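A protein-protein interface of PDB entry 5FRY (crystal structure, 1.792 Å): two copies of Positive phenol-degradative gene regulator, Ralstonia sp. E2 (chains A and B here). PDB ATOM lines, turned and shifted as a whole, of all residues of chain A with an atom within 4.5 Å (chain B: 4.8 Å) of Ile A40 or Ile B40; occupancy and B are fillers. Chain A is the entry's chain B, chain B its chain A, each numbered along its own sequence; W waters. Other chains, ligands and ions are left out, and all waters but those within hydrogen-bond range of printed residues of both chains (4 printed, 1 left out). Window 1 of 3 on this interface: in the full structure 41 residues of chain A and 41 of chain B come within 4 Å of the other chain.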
ATOM      1  N   MET A  39      15.269 -13.047  -2.384  1.00  0.00           N
ATOM      2  CA  MET A  39      14.738 -12.570  -1.114  1.00  0.00           C
ATOM      3  C   MET A  39      14.854 -13.679  -0.083  1.00  0.00           C
ATOM      4  O   MET A  39      14.960 -14.841  -0.454  1.00  0.00           O
ATOM      5  CB  MET A  39      13.268 -12.174  -1.258  1.00  0.00           C
ATOM      6  CG  MET A  39      12.944 -11.350  -2.518  1.00  0.00           C
ATOM      7  SD  MET A  39      13.537  -9.689  -2.402  1.00  0.00           S
ATOM      8  CE  MET A  39      12.346  -8.970  -1.276  1.00  0.00           C
ATOM      9  N   ILE A  40      14.776 -13.318   1.193  1.00  0.00           N
ATOM     10  CA  ILE A  40      14.572 -14.315   2.243  1.00  0.00           C
ATOM     11  C   ILE A  40      13.405 -13.883   3.088  1.00  0.00           C
ATOM     12  O   ILE A  40      13.038 -12.709   3.090  1.00  0.00           O
ATOM     13  CB  ILE A  40      15.800 -14.528   3.157  1.00  0.00           C
ATOM     14  CG1 ILE A  40      16.288 -13.206   3.767  1.00  0.00           C
ATOM     15  CG2 ILE A  40      16.914 -15.261   2.381  1.00  0.00           C
ATOM     16  CD1 ILE A  40      17.338 -13.409   4.897  1.00  0.00           C
ATOM     17  N   LEU A  41      12.788 -14.852   3.742  1.00  0.00           N
ATOM     18  CA  LEU A  41      11.804 -14.559   4.763  1.00  0.00           C
ATOM     19  C   LEU A  41      12.563 -14.496   6.068  1.00  0.00           C
ATOM     20  O   LEU A  41      13.220 -15.467   6.432  1.00  0.00           O
ATOM     21  CB  LEU A  41      10.717 -15.631   4.811  1.00  0.00           C
ATOM     22  CG  LEU A  41       9.615 -15.428   3.767  1.00  0.00           C
ATOM     23  CD1 LEU A  41       8.740 -16.649   3.689  1.00  0.00           C
ATOM     24  CD2 LEU A  41       8.774 -14.177   4.096  1.00  0.00           C
ATOM     25  N   LEU A  42      12.508 -13.351   6.739  1.00  0.00           N
ATOM     26  CA  LEU A  42      13.220 -13.150   7.997  1.00  0.00           C
ATOM     27  C   LEU A  42      12.250 -12.797   9.103  1.00  0.00           C
ATOM     28  O   LEU A  42      11.300 -12.067   8.876  1.00  0.00           O
ATOM     29  CB  LEU A  42      14.251 -12.033   7.850  1.00  0.00           C
ATOM     30  CG  LEU A  42      15.231 -11.901   9.005  1.00  0.00           C
ATOM     31  CD1 LEU A  42      15.919 -13.248   9.294  1.00  0.00           C
ATOM     32  CD2 LEU A  42      16.238 -10.837   8.664  1.00  0.00           C
ATOM     33  N   THR A  44      10.800 -10.884  12.079  1.00  0.00           N
ATOM     34  CA  THR A  44      10.964  -9.525  12.593  1.00  0.00           C
ATOM     35  C   THR A  44      11.671  -9.529  13.949  1.00  0.00           C
ATOM     36  O   THR A  44      12.514  -8.652  14.197  1.00  0.00           O
ATOM     37  CB  THR A  44       9.611  -8.752  12.709  1.00  0.00           C
ATOM     38  OG1 THR A  44       8.719  -9.422  13.610  1.00  0.00           O
ATOM     39  CG2 THR A  44       8.953  -8.620  11.338  1.00  0.00           C
ATOM     40  N   LEU A  47      15.368  -9.665  13.422  1.00  0.00           N
ATOM     41  CA  LEU A  47      15.924  -8.422  12.926  1.00  0.00           C
ATOM     42  C   LEU A  47      15.854  -7.386  14.054  1.00  0.00           C
ATOM     43  O   LEU A  47      16.766  -6.585  14.222  1.00  0.00           O
ATOM     44  CB  LEU A  47      15.202  -7.963  11.639  1.00  0.00           C
ATOM     45  CG  LEU A  47      15.950  -6.912  10.813  1.00  0.00           C
ATOM     46  CD1 LEU A  47      17.382  -7.320  10.564  1.00  0.00           C
ATOM     47  CD2 LEU A  47      15.253  -6.627   9.476  1.00  0.00           C
ATOM     48  N   GLU A 105       5.962  -7.115   0.773  1.00  0.00           N
ATOM     49  CA  GLU A 105       7.133  -7.558   1.492  1.00  0.00           C
ATOM     50  C   GLU A 105       6.840  -7.645   2.994  1.00  0.00           C
ATOM     51  O   GLU A 105       7.692  -8.079   3.769  1.00  0.00           O
ATOM     52  CB  GLU A 105       8.313  -6.632   1.213  1.00  0.00           C
ATOM     53  CG  GLU A 105       9.077  -6.982  -0.077  1.00  0.00           C
ATOM     54  CD  GLU A 105       9.761  -5.782  -0.737  1.00  0.00           C
ATOM     55  OE1 GLU A 105      10.055  -4.762  -0.067  1.00  0.00           O
ATOM     56  OE2 GLU A 105       9.978  -5.851  -1.962  1.00  0.00           O
ATOM     57  N   GLY A 106       5.627  -7.254   3.382  1.00  0.00           N
ATOM     58  CA  GLY A 106       5.167  -7.410   4.753  1.00  0.00           C
ATOM     59  C   GLY A 106       5.847  -6.441   5.695  1.00  0.00           C
ATOM     60  O   GLY A 106       5.820  -6.603   6.918  1.00  0.00           O
ATOM     61  N   VAL A 107       6.397  -5.382   5.120  1.00  0.00           N
ATOM     62  CA  VAL A 107       7.125  -4.397   5.895  1.00  0.00           C
ATOM     63  C   VAL A 107       6.147  -3.446   6.591  1.00  0.00           C
ATOM     64  O   VAL A 107       6.274  -3.161   7.785  1.00  0.00           O
ATOM     65  CB  VAL A 107       8.104  -3.628   4.991  1.00  0.00           C
ATOM     66  CG1 VAL A 107       8.505  -2.324   5.615  1.00  0.00           C
ATOM     67  CG2 VAL A 107       9.363  -4.500   4.649  1.00  0.00           C
ATOM     68  N   PHE A 134       6.241  -2.635  10.725  1.00  0.00           N
ATOM     69  CA  PHE A 134       6.890  -3.697  11.490  1.00  0.00           C
ATOM     70  C   PHE A 134       8.005  -3.108  12.322  1.00  0.00           C
ATOM     71  O   PHE A 134       8.286  -3.599  13.407  1.00  0.00           O
ATOM     72  CB  PHE A 134       7.435  -4.815  10.584  1.00  0.00           C
ATOM     73  CG  PHE A 134       8.856  -4.598  10.128  1.00  0.00           C
ATOM     74  CD1 PHE A 134       9.924  -5.009  10.911  1.00  0.00           C
ATOM     75  CD2 PHE A 134       9.115  -3.990   8.914  1.00  0.00           C
ATOM     76  CE1 PHE A 134      11.228  -4.784  10.493  1.00  0.00           C
ATOM     77  CE2 PHE A 134      10.405  -3.778   8.489  1.00  0.00           C
ATOM     78  CZ  PHE A 134      11.472  -4.191   9.296  1.00  0.00           C
ATOM     79  N   MET A 153      14.574   1.826   8.416  1.00  0.00           N
ATOM     80  CA  MET A 153      14.664   0.996   7.223  1.00  0.00           C
ATOM     81  C   MET A 153      13.531   1.269   6.249  1.00  0.00           C
ATOM     82  O   MET A 153      13.701   1.162   5.029  1.00  0.00           O
ATOM     83  CB  MET A 153      14.664  -0.467   7.623  1.00  0.00           C
ATOM     84  CG  MET A 153      14.726  -1.432   6.467  1.00  0.00           C
ATOM     85  SD  MET A 153      15.218  -3.059   7.093  1.00  0.00           S
ATOM     86  CE  MET A 153      13.936  -4.050   6.338  1.00  0.00           C
ATOM     87  N   ARG B  38       5.877 -12.867  13.068  1.00  0.00           N
ATOM     88  CA  ARG B  38       5.722 -11.998  11.922  1.00  0.00           C
ATOM     89  C   ARG B  38       7.026 -12.038  11.142  1.00  0.00           C
ATOM     90  O   ARG B  38       8.106 -12.092  11.736  1.00  0.00           O
ATOM     91  CB  ARG B  38       5.365 -10.586  12.360  1.00  0.00           C
ATOM     92  CG  ARG B  38       4.885  -9.699  11.236  1.00  0.00           C
ATOM     93  CD  ARG B  38       4.805  -8.228  11.646  1.00  0.00           C
ATOM     94  NE  ARG B  38       4.579  -7.412  10.465  1.00  0.00           N
ATOM     95  CZ  ARG B  38       4.197  -6.143  10.464  1.00  0.00           C
ATOM     96  NH1 ARG B  38       3.990  -5.492  11.611  1.00  0.00           N
ATOM     97  NH2 ARG B  38       4.018  -5.524   9.302  1.00  0.00           N
ATOM     98  N   MET B  39       6.915 -12.069   9.819  1.00  0.00           N
ATOM     99  CA  MET B  39       8.078 -12.118   8.922  1.00  0.00           C
ATOM    100  C   MET B  39       8.099 -10.910   7.973  1.00  0.00           C
ATOM    101  O   MET B  39       7.065 -10.301   7.696  1.00  0.00           O
ATOM    102  CB  MET B  39       8.069 -13.401   8.081  1.00  0.00           C
ATOM    103  CG  MET B  39       7.729 -14.696   8.854  1.00  0.00           C
ATOM    104  SD  MET B  39       9.010 -15.190  10.005  1.00  0.00           S
ATOM    105  CE  MET B  39      10.169 -15.885   8.837  1.00  0.00           C
ATOM    106  N   ILE B  40       9.275 -10.584   7.449  1.00  0.00           N
ATOM    107  CA  ILE B  40       9.337  -9.732   6.264  1.00  0.00           C
ATOM    108  C   ILE B  40      10.093 -10.437   5.165  1.00  0.00           C
ATOM    109  O   ILE B  40      10.894 -11.353   5.439  1.00  0.00           O
ATOM    110  CB  ILE B  40      10.016  -8.360   6.505  1.00  0.00           C
ATOM    111  CG1 ILE B  40      11.444  -8.526   7.022  1.00  0.00           C
ATOM    112  CG2 ILE B  40       9.201  -7.516   7.480  1.00  0.00           C
ATOM    113  CD1 ILE B  40      12.189  -7.221   6.987  1.00  0.00           C
ATOM    114  N   LEU B  41       9.818 -10.028   3.924  1.00  0.00           N
ATOM    115  CA  LEU B  41      10.669 -10.409   2.783  1.00  0.00           C
ATOM    116  C   LEU B  41      11.745  -9.360   2.636  1.00  0.00           C
ATOM    117  O   LEU B  41      11.432  -8.176   2.481  1.00  0.00           O
ATOM    118  CB  LEU B  41       9.862 -10.506   1.487  1.00  0.00           C
ATOM    119  CG  LEU B  41       8.888 -11.675   1.321  1.00  0.00           C
ATOM    120  CD1 LEU B  41       7.819 -11.316   0.284  1.00  0.00           C
ATOM    121  CD2 LEU B  41       9.605 -12.954   0.944  1.00  0.00           C
ATOM    122  N   LEU B  42      13.004  -9.779   2.664  1.00  0.00           N
ATOM    123  CA  LEU B  42      14.108  -8.830   2.612  1.00  0.00           C
ATOM    124  C   LEU B  42      15.050  -9.193   1.479  1.00  0.00           C
ATOM    125  O   LEU B  42      15.364 -10.341   1.323  1.00  0.00           O
ATOM    126  CB  LEU B  42      14.864  -8.814   3.949  1.00  0.00           C
ATOM    127  CG  LEU B  42      15.979  -7.784   4.074  1.00  0.00           C
ATOM    128  CD1 LEU B  42      15.426  -6.381   3.958  1.00  0.00           C
ATOM    129  CD2 LEU B  42      16.685  -7.969   5.427  1.00  0.00           C
ATOM    130  N   THR B  44      18.205 -10.080  -0.469  1.00  0.00           N
ATOM    131  CA  THR B  44      19.484 -10.581   0.005  1.00  0.00           C
ATOM    132  C   THR B  44      20.564  -9.542  -0.255  1.00  0.00           C
ATOM    133  O   THR B  44      21.520  -9.458   0.484  1.00  0.00           O
ATOM    134  CB  THR B  44      19.860 -11.897  -0.665  1.00  0.00           C
ATOM    135  OG1 THR B  44      20.020 -11.676  -2.075  1.00  0.00           O
ATOM    136  CG2 THR B  44      18.769 -12.933  -0.432  1.00  0.00           C
ATOM    137  N   LEU B  47      20.736  -7.218   2.620  1.00  0.00           N
ATOM    138  CA  LEU B  47      21.438  -7.807   3.752  1.00  0.00           C
ATOM    139  C   LEU B  47      22.947  -7.756   3.502  1.00  0.00           C
ATOM    140  O   LEU B  47      23.729  -7.484   4.415  1.00  0.00           O
ATOM    141  CB  LEU B  47      20.979  -9.241   4.000  1.00  0.00           C
ATOM    142  CG  LEU B  47      20.122  -9.430   5.259  1.00  0.00           C
ATOM    143  CD1 LEU B  47      19.804 -10.890   5.497  1.00  0.00           C
ATOM    144  CD2 LEU B  47      20.789  -8.818   6.473  1.00  0.00           C
ATOM    145  N   GLU B 105      11.954 -20.480   3.860  1.00  0.00           N
ATOM    146  CA  GLU B 105      12.381 -19.111   4.091  1.00  0.00           C
ATOM    147  C   GLU B 105      13.350 -18.628   3.009  1.00  0.00           C
ATOM    148  O   GLU B 105      13.798 -17.478   3.038  1.00  0.00           O
ATOM    149  CB  GLU B 105      13.003 -18.991   5.499  1.00  0.00           C
ATOM    150  CG  GLU B 105      11.938 -19.066   6.585  1.00  0.00           C
ATOM    151  CD  GLU B 105      12.446 -19.397   7.968  1.00  0.00           C
ATOM    152  OE1 GLU B 105      13.668 -19.280   8.283  1.00  0.00           O
ATOM    153  OE2 GLU B 105      11.591 -19.815   8.765  1.00  0.00           O
ATOM    154  N   GLY B 106      13.654 -19.498   2.039  1.00  0.00           N
ATOM    155  CA  GLY B 106      14.510 -19.137   0.913  1.00  0.00           C
ATOM    156  C   GLY B 106      15.955 -18.870   1.299  1.00  0.00           C
ATOM    157  O   GLY B 106      16.670 -18.139   0.628  1.00  0.00           O
ATOM    158  N   VAL B 107      16.393 -19.465   2.397  1.00  0.00           N
ATOM    159  CA  VAL B 107      17.748 -19.252   2.887  1.00  0.00           C
ATOM    160  C   VAL B 107      18.759 -20.178   2.215  1.00  0.00           C
ATOM    161  O   VAL B 107      19.857 -19.759   1.808  1.00  0.00           O
ATOM    162  CB  VAL B 107      17.805 -19.472   4.422  1.00  0.00           C
ATOM    163  CG1 VAL B 107      19.224 -19.628   4.889  1.00  0.00           C
ATOM    164  CG2 VAL B 107      17.103 -18.299   5.168  1.00  0.00           C
ATOM    165  N   PHE B 134      22.167 -18.792   0.419  1.00  0.00           N
ATOM    166  CA  PHE B 134      22.102 -17.403  -0.017  1.00  0.00           C
ATOM    167  C   PHE B 134      23.274 -16.631   0.567  1.00  0.00           C
ATOM    168  O   PHE B 134      23.807 -15.709  -0.040  1.00  0.00           O
ATOM    169  CB  PHE B 134      20.796 -16.751   0.421  1.00  0.00           C
ATOM    170  CG  PHE B 134      20.896 -16.061   1.743  1.00  0.00           C
ATOM    171  CD1 PHE B 134      20.787 -16.781   2.921  1.00  0.00           C
ATOM    172  CD2 PHE B 134      21.159 -14.703   1.815  1.00  0.00           C
ATOM    173  CE1 PHE B 134      20.901 -16.160   4.144  1.00  0.00           C
ATOM    174  CE2 PHE B 134      21.284 -14.068   3.045  1.00  0.00           C
ATOM    175  CZ  PHE B 134      21.157 -14.794   4.206  1.00  0.00           C
HETATM  176  O   HOH W   1      15.794 -17.051  -1.427  1.00  0.00           O
HETATM  177  O   HOH W   2       4.923  -8.883   8.194  1.00  0.00           O
HETATM  178  O   HOH W   3      11.993  -5.589   2.250  1.00  0.00           O
HETATM  179  O   HOH W   4      14.969 -17.084   7.859  1.00  0.00           O
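O of Arg B38 lies within hydrogen-bond range of N of Thr A44, 3.0 Å away. The backbone carbonyl oxygen (O) of Gly A106 sits at hydrogen-bond distance from the guanidinium group (NH2) of Arg B38 (3.2 Å). O of Ile B40 is in hydrogen-bond range of N of Leu A42. N of Leu B41 lies within hydrogen-bond range of O of Glu A105 (2.9 Å). O of Ile A40 is in hydrogen-bond range of N of Leu B42 (3.0 Å). The backbone NH (N) of Leu A41 lies within hydrogen-bond range of the backbone carbonyl oxygen (O) of Glu B105 (2.9 Å). O of Ile A40 sits close to O of Ile B40 (3.5 Å).
The backbone NH (N) of Phe A134 is in hydrogen-bond range of the backbone carbonyl oxygen (O) of Val A107.
Among the printed residues, pairs that only touch across the chains: Leu A42 with Met B39, Ile A40 with Leu B41, Ile A40 with Glu B105, Met A39 with Leu B42, Ile A40 with Gly B106, Leu A41 with Ile B40, Phe A134 with Arg B38, Glu A105 with Ile B40, Leu A41 with Leu B41, Gly A106 with Ile B40, Ile A40 with Leu B47, Val A107 with Arg B38, Met A153 with Leu B42, Met A153 with Ile B40, Phe A134 with Ile B40, Met A39 with Gly B106, Leu A41 with Met B39, Met A39 with Leu B41, Gly A106 with Met B39 and Leu A47 with Ile B40.
Of chain B, only Ile B40, Leu B41, Leu B42, Leu B47, Glu B105 and Gly B106 come within 4 Å of Ile A40. Of the printed residues of chain A, Ile B40 touches Ile A40 (3.5 Å), Leu A41 (3.4 Å), Leu A42 (2.9 Å), Leu A47 (3.99 Å), Glu A105 (3.4 Å), Gly A106 (3.5 Å), Phe A134 (3.8 Å) and Met A153 (3.7 Å). Of the printed residues of chain B, Leu A41 touches Met B39 (3.9 Å), Ile B40 (3.4 Å), Leu B41 (3.5 Å) and Glu B105 (2.9 Å). Printed residues of chain A within 4 Å of Leu B41: Met A39, Ile A40, Leu A41 and Glu A105. Of the printed residues of chain B, Phe A134 touches Arg B38 (3.4 Å) and Ile B40 (3.8 Å). Printed residues of chain B within 4 Å of Leu A47: Ile B40 (3.99 Å). The nearest printed residue of chain B that does not touch Ile A40 is Thr B44 (4.1 Å).
Of the 11 printed residues of chain A, 11 touch a printed residue of chain B. Printed residues of chain A that touch a printed residue of chain B: Met A39, Ile A40, Leu A41, Leu A42, Thr A44, Leu A47, Glu A105, Gly A106, Val A107, Phe A134 and Met A153. Hydrophobic or aromatic side chains of chain A that line the printed part of chain B: Met A39, Ile A40, Leu A41, Leu A47, Phe A134 and Met A153. Of the 11 printed residues of chain B, 8 touch a printed residue of chain A. Hydrophobic or aromatic side chains of chain B within 4 Å of the printed part of chain A: Met B39, Ile B40, Leu B41, Leu B42 and Leu B47. Among the printed residues, 27 pairs touch across the chains.
Met A39 touches Leu B41, and with the chains exchanged Leu A41 touches Met B39. Ile B40 touches its own counterpart, Ile A40. Ile A40 touches Leu B41, and with the chains exchanged Leu A41 touches Ile B40. Ile A40 touches Gly B106, and with the chains exchanged Gly A106 touches Ile B40. 10 positions are printed for both chains. Of the 27 pairs that touch across the chains among the printed residues, 20 have their exchanged pair printed and touching as well.
Water W1 lies within hydrogen-bond range of O of Gly B106 (2.5 Å) and O of Met A39 (2.6 Å). Water W4 lies within hydrogen-bond range of OE1 of Glu B105 (2.6 Å) and O of Leu A41 (2.8 Å). Water W2 lies within hydrogen-bond range of the backbone carbonyl oxygen (O) of Met B39 (2.6 Å), the guanidinium group (NE) of Arg B38 (2.7 Å) and the backbone carbonyl oxygen (O) of Gly A106 (2.8 Å). Water W3 lies within hydrogen-bond range of O of Leu B41 (2.7 Å) and OE1 of Glu A105 (3.1 Å).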
